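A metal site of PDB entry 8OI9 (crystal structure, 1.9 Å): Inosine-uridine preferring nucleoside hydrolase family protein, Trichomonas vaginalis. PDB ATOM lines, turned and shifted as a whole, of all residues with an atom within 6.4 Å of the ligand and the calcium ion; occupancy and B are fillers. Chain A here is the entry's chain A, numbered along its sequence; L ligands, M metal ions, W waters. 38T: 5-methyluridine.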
ATOM      1  N   CYS A   9      16.398 -22.275 -25.878  1.00  0.00           N
ATOM      2  CA  CYS A   9      15.951 -20.881 -25.895  1.00  0.00           C
ATOM      3  C   CYS A   9      17.051 -19.919 -25.456  1.00  0.00           C
ATOM      4  O   CYS A   9      18.147 -20.338 -25.084  1.00  0.00           O
ATOM      5  CB  CYS A   9      14.707 -20.743 -25.025  1.00  0.00           C
ATOM      6  SG  CYS A   9      14.990 -21.286 -23.317  1.00  0.00           S
ATOM      7  N   ASP A  10      16.748 -18.613 -25.521  1.00  0.00           N
ATOM      8  CA  ASP A  10      17.681 -17.543 -25.193  1.00  0.00           C
ATOM      9  C   ASP A  10      17.009 -16.434 -24.378  1.00  0.00           C
ATOM     10  O   ASP A  10      16.929 -15.286 -24.819  1.00  0.00           O
ATOM     11  CB  ASP A  10      18.260 -16.926 -26.478  1.00  0.00           C
ATOM     12  CG  ASP A  10      17.216 -16.284 -27.382  1.00  0.00           C
ATOM     13  OD1 ASP A  10      16.004 -16.628 -27.239  1.00  0.00           O
ATOM     14  OD2 ASP A  10      17.610 -15.413 -28.196  1.00  0.00           O
ATOM     15  N   PRO A  11      16.520 -16.702 -23.149  1.00  0.00           N
ATOM     16  CA  PRO A  11      15.739 -15.721 -22.411  1.00  0.00           C
ATOM     17  C   PRO A  11      16.522 -14.458 -22.055  1.00  0.00           C
ATOM     18  O   PRO A  11      17.651 -14.575 -21.569  1.00  0.00           O
ATOM     19  CB  PRO A  11      15.308 -16.409 -21.107  1.00  0.00           C
ATOM     20  CG  PRO A  11      15.919 -17.791 -21.135  1.00  0.00           C
ATOM     21  CD  PRO A  11      16.662 -17.976 -22.428  1.00  0.00           C
ATOM     22  N   GLY A  12      15.966 -13.264 -22.320  1.00  0.00           N
ATOM     23  CA  GLY A  12      14.825 -13.040 -23.188  1.00  0.00           C
ATOM     24  C   GLY A  12      13.480 -13.119 -22.454  1.00  0.00           C
ATOM     25  O   GLY A  12      13.162 -14.147 -21.865  1.00  0.00           O
ATOM     26  N   HIS A  13      12.697 -12.029 -22.538  1.00  0.00           N
ATOM     27  CA  HIS A  13      11.406 -11.909 -21.865  1.00  0.00           C
ATOM     28  C   HIS A  13      10.387 -12.880 -22.454  1.00  0.00           C
ATOM     29  O   HIS A  13       9.611 -13.479 -21.728  1.00  0.00           O
ATOM     30  CB  HIS A  13      10.871 -10.475 -21.957  1.00  0.00           C
ATOM     31  CG  HIS A  13      11.783  -9.450 -21.380  1.00  0.00           C
ATOM     32  ND1 HIS A  13      13.004  -9.111 -21.933  1.00  0.00           N
ATOM     33  CD2 HIS A  13      11.654  -8.684 -20.279  1.00  0.00           C
ATOM     34  CE1 HIS A  13      13.580  -8.178 -21.189  1.00  0.00           C
ATOM     35  NE2 HIS A  13      12.777  -7.900 -20.175  1.00  0.00           N
ATOM     36  N   ASP A  14      10.382 -12.990 -23.789  1.00  0.00           N
ATOM     37  CA  ASP A  14       9.524 -13.909 -24.506  1.00  0.00           C
ATOM     38  C   ASP A  14       9.799 -15.350 -24.058  1.00  0.00           C
ATOM     39  O   ASP A  14       8.863 -16.116 -23.804  1.00  0.00           O
ATOM     40  CB  ASP A  14       9.742 -13.794 -26.017  1.00  0.00           C
ATOM     41  CG  ASP A  14       9.317 -12.448 -26.566  1.00  0.00           C
ATOM     42  OD1 ASP A  14       8.078 -12.249 -26.725  1.00  0.00           O
ATOM     43  OD2 ASP A  14      10.209 -11.574 -26.789  1.00  0.00           O
ATOM     44  N   ASP A  15      11.077 -15.707 -23.998  1.00  0.00           N
ATOM     45  CA  ASP A  15      11.482 -17.064 -23.671  1.00  0.00           C
ATOM     46  C   ASP A  15      11.060 -17.369 -22.234  1.00  0.00           C
ATOM     47  O   ASP A  15      10.649 -18.496 -21.941  1.00  0.00           O
ATOM     48  CB  ASP A  15      12.979 -17.285 -23.878  1.00  0.00           C
ATOM     49  CG  ASP A  15      13.516 -16.833 -25.234  1.00  0.00           C
ATOM     50  OD1 ASP A  15      13.640 -15.613 -25.455  1.00  0.00           O
ATOM     51  OD2 ASP A  15      13.814 -17.702 -26.052  1.00  0.00           O
ATOM     52  N   GLY A  38      22.350 -15.169 -28.079  1.00  0.00           N
ATOM     53  CA  GLY A  38      21.429 -14.300 -28.784  1.00  0.00           C
ATOM     54  C   GLY A  38      21.923 -12.854 -28.724  1.00  0.00           C
ATOM     55  O   GLY A  38      23.098 -12.568 -28.994  1.00  0.00           O
ATOM     56  N   ASN A  39      21.007 -11.949 -28.362  1.00  0.00           N
ATOM     57  CA  ASN A  39      21.329 -10.574 -28.016  1.00  0.00           C
ATOM     58  C   ASN A  39      22.306 -10.516 -26.845  1.00  0.00           C
ATOM     59  O   ASN A  39      23.128  -9.598 -26.782  1.00  0.00           O
ATOM     60  CB  ASN A  39      20.098  -9.764 -27.621  1.00  0.00           C
ATOM     61  CG  ASN A  39      19.619  -8.840 -28.711  1.00  0.00           C
ATOM     62  OD1 ASN A  39      20.358  -8.532 -29.643  1.00  0.00           O
ATOM     63  ND2 ASN A  39      18.380  -8.373 -28.587  1.00  0.00           N
ATOM     64  N   THR A 142      13.250 -21.582 -29.447  1.00  0.00           N
ATOM     65  CA  THR A 142      12.765 -20.210 -29.494  1.00  0.00           C
ATOM     66  C   THR A 142      13.914 -19.192 -29.466  1.00  0.00           C
ATOM     67  O   THR A 142      13.675 -18.037 -29.185  1.00  0.00           O
ATOM     68  CB  THR A 142      11.751 -19.938 -28.380  1.00  0.00           C
ATOM     69  OG1 THR A 142      12.402 -19.974 -27.108  1.00  0.00           O
ATOM     70  CG2 THR A 142      10.589 -20.899 -28.399  1.00  0.00           C
ATOM     71  N   GLY A 143      15.130 -19.615 -29.807  1.00  0.00           N
ATOM     72  CA  GLY A 143      16.243 -18.716 -30.083  1.00  0.00           C
ATOM     73  C   GLY A 143      16.957 -19.157 -31.350  1.00  0.00           C
ATOM     74  O   GLY A 143      16.356 -19.800 -32.183  1.00  0.00           O
ATOM     75  N   MET A 167       9.739 -21.078 -32.701  1.00  0.00           N
ATOM     76  CA  MET A 167       9.442 -19.694 -32.991  1.00  0.00           C
ATOM     77  C   MET A 167      10.604 -19.187 -33.822  1.00  0.00           C
ATOM     78  O   MET A 167      11.744 -19.154 -33.347  1.00  0.00           O
ATOM     79  CB  MET A 167       9.286 -18.892 -31.701  1.00  0.00           C
ATOM     80  CG  MET A 167       8.787 -17.469 -31.911  1.00  0.00           C
ATOM     81  SD  MET A 167      10.063 -16.346 -32.511  1.00  0.00           S
ATOM     82  CE  MET A 167       9.243 -15.654 -33.955  1.00  0.00           C
ATOM     83  N   ASN A 176      12.015  -8.362 -38.756  1.00  0.00           N
ATOM     84  CA  ASN A 176      12.064  -7.413 -37.652  1.00  0.00           C
ATOM     85  C   ASN A 176      13.432  -6.752 -37.620  1.00  0.00           C
ATOM     86  O   ASN A 176      13.556  -5.582 -37.963  1.00  0.00           O
ATOM     87  CB  ASN A 176      11.585  -8.033 -36.327  1.00  0.00           C
ATOM     88  CG  ASN A 176      12.210  -9.340 -35.909  1.00  0.00           C
ATOM     89  OD1 ASN A 176      13.265  -9.749 -36.390  1.00  0.00           O
ATOM     90  ND2 ASN A 176      11.580 -10.000 -34.946  1.00  0.00           N
ATOM     91  N   ILE A 177      14.473  -7.500 -37.237  1.00  0.00           N
ATOM     92  CA  ILE A 177      15.805  -6.960 -37.029  1.00  0.00           C
ATOM     93  C   ILE A 177      16.477  -6.650 -38.373  1.00  0.00           C
ATOM     94  O   ILE A 177      17.344  -5.780 -38.431  1.00  0.00           O
ATOM     95  CB  ILE A 177      16.617  -7.934 -36.149  1.00  0.00           C
ATOM     96  CG1 ILE A 177      16.064  -7.947 -34.723  1.00  0.00           C
ATOM     97  CG2 ILE A 177      18.109  -7.605 -36.158  1.00  0.00           C
ATOM     98  CD1 ILE A 177      16.152  -6.601 -34.022  1.00  0.00           C
ATOM     99  N   GLU A 182      13.899 -12.649 -39.769  1.00  0.00           N
ATOM    100  CA  GLU A 182      13.584 -12.663 -38.355  1.00  0.00           C
ATOM    101  C   GLU A 182      14.840 -13.033 -37.567  1.00  0.00           C
ATOM    102  O   GLU A 182      15.671 -13.818 -38.034  1.00  0.00           O
ATOM    103  CB  GLU A 182      12.410 -13.629 -38.170  1.00  0.00           C
ATOM    104  CG  GLU A 182      11.954 -13.820 -36.744  1.00  0.00           C
ATOM    105  CD  GLU A 182      12.806 -14.792 -35.947  1.00  0.00           C
ATOM    106  OE1 GLU A 182      13.244 -15.824 -36.547  1.00  0.00           O
ATOM    107  OE2 GLU A 182      13.028 -14.519 -34.741  1.00  0.00           O
ATOM    108  N   PHE A 183      14.931 -12.483 -36.356  1.00  0.00           N
ATOM    109  CA  PHE A 183      16.129 -12.525 -35.522  1.00  0.00           C
ATOM    110  C   PHE A 183      16.681 -13.947 -35.356  1.00  0.00           C
ATOM    111  O   PHE A 183      17.872 -14.191 -35.573  1.00  0.00           O
ATOM    112  CB  PHE A 183      15.817 -11.906 -34.166  1.00  0.00           C
ATOM    113  CG  PHE A 183      16.981 -11.829 -33.214  1.00  0.00           C
ATOM    114  CD1 PHE A 183      18.035 -10.967 -33.466  1.00  0.00           C
ATOM    115  CD2 PHE A 183      17.038 -12.651 -32.104  1.00  0.00           C
ATOM    116  CE1 PHE A 183      19.117 -10.897 -32.593  1.00  0.00           C
ATOM    117  CE2 PHE A 183      18.110 -12.578 -31.228  1.00  0.00           C
ATOM    118  CZ  PHE A 183      19.153 -11.710 -31.487  1.00  0.00           C
ATOM    119  N   ASN A 184      15.823 -14.871 -34.910  1.00  0.00           N
ATOM    120  CA  ASN A 184      16.253 -16.233 -34.602  1.00  0.00           C
ATOM    121  C   ASN A 184      16.895 -16.931 -35.812  1.00  0.00           C
ATOM    122  O   ASN A 184      17.833 -17.698 -35.625  1.00  0.00           O
ATOM    123  CB  ASN A 184      15.116 -17.085 -34.039  1.00  0.00           C
ATOM    124  CG  ASN A 184      14.698 -16.616 -32.661  1.00  0.00           C
ATOM    125  OD1 ASN A 184      15.410 -15.844 -32.018  1.00  0.00           O
ATOM    126  ND2 ASN A 184      13.533 -17.052 -32.214  1.00  0.00           N
ATOM    127  N   LEU A 208       6.680 -14.657 -37.332  1.00  0.00           N
ATOM    128  CA  LEU A 208       6.166 -13.318 -37.062  1.00  0.00           C
ATOM    129  C   LEU A 208       4.735 -13.188 -37.582  1.00  0.00           C
ATOM    130  O   LEU A 208       3.936 -12.451 -36.998  1.00  0.00           O
ATOM    131  CB  LEU A 208       7.086 -12.268 -37.708  1.00  0.00           C
ATOM    132  CG  LEU A 208       8.530 -12.235 -37.207  1.00  0.00           C
ATOM    133  CD1 LEU A 208       9.241 -11.010 -37.786  1.00  0.00           C
ATOM    134  CD2 LEU A 208       8.602 -12.246 -35.678  1.00  0.00           C
ATOM    135  N   THR A 211       2.969 -14.312 -34.488  1.00  0.00           N
ATOM    136  CA  THR A 211       3.308 -13.661 -33.218  1.00  0.00           C
ATOM    137  C   THR A 211       3.008 -12.166 -33.250  1.00  0.00           C
ATOM    138  O   THR A 211       2.701 -11.592 -32.208  1.00  0.00           O
ATOM    139  CB  THR A 211       4.763 -13.937 -32.822  1.00  0.00           C
ATOM    140  OG1 THR A 211       5.664 -13.303 -33.738  1.00  0.00           O
ATOM    141  CG2 THR A 211       5.062 -15.422 -32.734  1.00  0.00           C
ATOM    142  N   PHE A 246       9.745  -3.635 -23.413  1.00  0.00           N
ATOM    143  CA  PHE A 246      10.148  -3.132 -24.724  1.00  0.00           C
ATOM    144  C   PHE A 246       8.971  -2.484 -25.468  1.00  0.00           C
ATOM    145  O   PHE A 246       9.040  -2.309 -26.682  1.00  0.00           O
ATOM    146  CB  PHE A 246      10.765  -4.273 -25.546  1.00  0.00           C
ATOM    147  CG  PHE A 246      12.148  -4.665 -25.093  1.00  0.00           C
ATOM    148  CD1 PHE A 246      13.214  -3.791 -25.217  1.00  0.00           C
ATOM    149  CD2 PHE A 246      12.374  -5.909 -24.511  1.00  0.00           C
ATOM    150  CE1 PHE A 246      14.477  -4.153 -24.792  1.00  0.00           C
ATOM    151  CE2 PHE A 246      13.644  -6.272 -24.098  1.00  0.00           C
ATOM    152  CZ  PHE A 246      14.693  -5.398 -24.239  1.00  0.00           C
ATOM    153  N   THR A 249       9.842   0.753 -27.504  1.00  0.00           N
ATOM    154  CA  THR A 249      10.649   0.427 -28.662  1.00  0.00           C
ATOM    155  C   THR A 249       9.786  -0.224 -29.758  1.00  0.00           C
ATOM    156  O   THR A 249       9.913   0.094 -30.931  1.00  0.00           O
ATOM    157  CB  THR A 249      11.825  -0.463 -28.267  1.00  0.00           C
ATOM    158  OG1 THR A 249      11.326  -1.605 -27.584  1.00  0.00           O
ATOM    159  CG2 THR A 249      12.817   0.248 -27.375  1.00  0.00           C
ATOM    160  N   TYR A 250       8.905  -1.140 -29.358  1.00  0.00           N
ATOM    161  CA  TYR A 250       7.975  -1.744 -30.296  1.00  0.00           C
ATOM    162  C   TYR A 250       7.070  -0.671 -30.913  1.00  0.00           C
ATOM    163  O   TYR A 250       6.778  -0.723 -32.111  1.00  0.00           O
ATOM    164  CB  TYR A 250       7.172  -2.849 -29.608  1.00  0.00           C
ATOM    165  CG  TYR A 250       7.801  -4.218 -29.625  1.00  0.00           C
ATOM    166  CD1 TYR A 250       8.020  -4.879 -30.822  1.00  0.00           C
ATOM    167  CD2 TYR A 250       8.130  -4.875 -28.443  1.00  0.00           C
ATOM    168  CE1 TYR A 250       8.576  -6.151 -30.858  1.00  0.00           C
ATOM    169  CE2 TYR A 250       8.691  -6.141 -28.468  1.00  0.00           C
ATOM    170  CZ  TYR A 250       8.903  -6.787 -29.669  1.00  0.00           C
ATOM    171  OH  TYR A 250       9.443  -8.044 -29.697  1.00  0.00           O
ATOM    172  N   HIS A 262       6.101 -13.639 -28.415  1.00  0.00           N
ATOM    173  CA  HIS A 262       6.492 -14.543 -29.490  1.00  0.00           C
ATOM    174  C   HIS A 262       6.544 -15.989 -28.981  1.00  0.00           C
ATOM    175  O   HIS A 262       5.658 -16.782 -29.259  1.00  0.00           O
ATOM    176  CB  HIS A 262       7.859 -14.135 -30.066  1.00  0.00           C
ATOM    177  CG  HIS A 262       7.961 -12.768 -30.634  1.00  0.00           C
ATOM    178  ND1 HIS A 262       7.498 -12.426 -31.890  1.00  0.00           N
ATOM    179  CD2 HIS A 262       8.551 -11.667 -30.143  1.00  0.00           C
ATOM    180  CE1 HIS A 262       7.778 -11.154 -32.120  1.00  0.00           C
ATOM    181  NE2 HIS A 262       8.403 -10.666 -31.061  1.00  0.00           N
ATOM    182  N   ASP A 263       7.584 -16.277 -28.194  1.00  0.00           N
ATOM    183  CA  ASP A 263       8.063 -17.636 -27.939  1.00  0.00           C
ATOM    184  C   ASP A 263       7.001 -18.556 -27.349  1.00  0.00           C
ATOM    185  O   ASP A 263       6.918 -19.718 -27.740  1.00  0.00           O
ATOM    186  CB  ASP A 263       9.323 -17.589 -27.071  1.00  0.00           C
ATOM    187  CG  ASP A 263      10.467 -16.902 -27.792  1.00  0.00           C
ATOM    188  OD1 ASP A 263      10.293 -16.555 -28.973  1.00  0.00           O
ATOM    189  OD2 ASP A 263      11.521 -16.705 -27.163  1.00  0.00           O
HETATM  190  OAC 38T L   1      16.131 -11.674 -28.316  1.00  0.00           O
HETATM  191  CAM 38T L   1      15.251 -10.828 -28.364  1.00  0.00           C
HETATM  192  NAI 38T L   1      15.437  -9.576 -27.810  1.00  0.00           N
HETATM  193  CAL 38T L   1      14.547  -8.523 -27.784  1.00  0.00           C
HETATM  194  OAB 38T L   1      14.852  -7.464 -27.251  1.00  0.00           O
HETATM  195  CAK 38T L   1      13.270  -8.798 -28.417  1.00  0.00           C
HETATM  196  CAA 38T L   1      12.237  -7.705 -28.432  1.00  0.00           C
HETATM  197  CAG 38T L   1      13.058 -10.011 -28.954  1.00  0.00           C
HETATM  198  NAR 38T L   1      14.016 -11.020 -28.950  1.00  0.00           N
HETATM  199  C1' 38T L   1      13.717 -12.353 -29.534  1.00  0.00           C
HETATM  200  O4' 38T L   1      13.410 -12.212 -30.896  1.00  0.00           O
HETATM  201  C4' 38T L   1      12.618 -13.359 -31.322  1.00  0.00           C
HETATM  202  C5' 38T L   1      11.593 -12.899 -32.329  1.00  0.00           C
HETATM  203  O5' 38T L   1      12.215 -12.467 -33.539  1.00  0.00           O
HETATM  204  C3' 38T L   1      12.010 -13.964 -30.038  1.00  0.00           C
HETATM  205  O3' 38T L   1      12.415 -15.304 -29.793  1.00  0.00           O
HETATM  206  C2' 38T L   1      12.484 -13.038 -28.921  1.00  0.00           C
HETATM  207  O2' 38T L   1      12.903 -13.791 -27.809  1.00  0.00           O
HETATM  208 CA    CA M   1      13.728 -16.046 -27.858  1.00  0.00          CA
HETATM  209  O   HOH W   1      18.596 -13.041 -27.674  1.00  0.00           O
HETATM  210  O   HOH W   2      12.460 -11.988 -25.730  1.00  0.00           O
HETATM  211  O   HOH W   3      15.492 -13.640 -26.521  1.00  0.00           O
HETATM  212  O   HOH W   4      15.310 -15.225 -29.493  1.00  0.00           O
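ND2 of Asn 184 lies close to O3' of the ligand, 3.2 Å away.
ND2 of Asn 176 lies within hydrogen-bond range of O5' of the ligand, at 2.9 Å.
OE2 of Glu 182 sits at hydrogen-bond distance from O5' of the ligand (2.5 Å).
SD of Met 167 sits close to O3' of the ligand, 3.7 Å away.
NAI of the ligand lies close to ND2 of Asn 39 (3.3 Å).
O of Phe 246 sits at hydrogen-bond distance from OG1 of Thr 249.
The side-chain carboxylate (OD1) of Asp 14 lies within hydrogen-bond range of the backbone NH (N) of His 262, 2.9 Å away.
The backbone NH of Phe 183 sits at hydrogen-bond distance from the side-chain amide oxygen of Asn 176 (3.2 Å).
A ring nitrogen (ND1) of His 262 is in hydrogen-bond range of the side-chain hydroxyl of Thr 211, 2.7 Å away.
The side-chain hydroxyl of Tyr 250 lies within hydrogen-bond range of a ring nitrogen (NE2) of His 262 (3.1 Å).
The backbone carbonyl oxygen of Thr 142 lies close to the side-chain amide nitrogen of Asn 184.
The side-chain carboxylate (OE2) of Glu 182 is in hydrogen-bond range of the backbone NH (N) of Asn 184 (2.8 Å).
ND2 of Asn 184 sits at hydrogen-bond distance from O of Met 167, 3.0 Å away.
Residues that only touch the ligand: Tyr 250 (3.1 Å), Asp 14 (3.4 Å), Phe 246 (3.6 Å), Phe 183 (3.6 Å) and His 262 (3.9 Å).
Within 4 Å of the calcium ion: Asp 10, Asp 15, Thr 142 and Asp 263.
The nearest printed residue that does not touch the calcium ion is Gly 143 (4.3 Å).
The calcium ion is bound by O of Thr 142 (2.4 Å), O2' of the ligand (2.4 Å), OD2 of Asp 263 (2.4 Å), water W4 (2.4 Å), OD1 of Asp 10 (2.4 Å), OD1 of Asp 15 (2.4 Å), OD2 of Asp 15 (2.5 Å) and O3' of the ligand (2.5 Å).
Water W4 bridges the side-chain amide oxygen of Asn 184 (2.6 Å) and the side-chain carboxylate of Asp 10 (2.6 Å).
Water W3 bridges an oxygen (OAC) of the ligand (2.7 Å) and the backbone carbonyl oxygen of Asp 10 (2.8 Å).
Water W2 bridges the side-chain carboxylate of Asp 14 and the backbone NH of His 13.
Water W1 lies within hydrogen-bond range of OD2 of Asp 10 (2.6 Å), N of Asn 39 (2.7 Å) and OAC of the ligand (2.9 Å).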
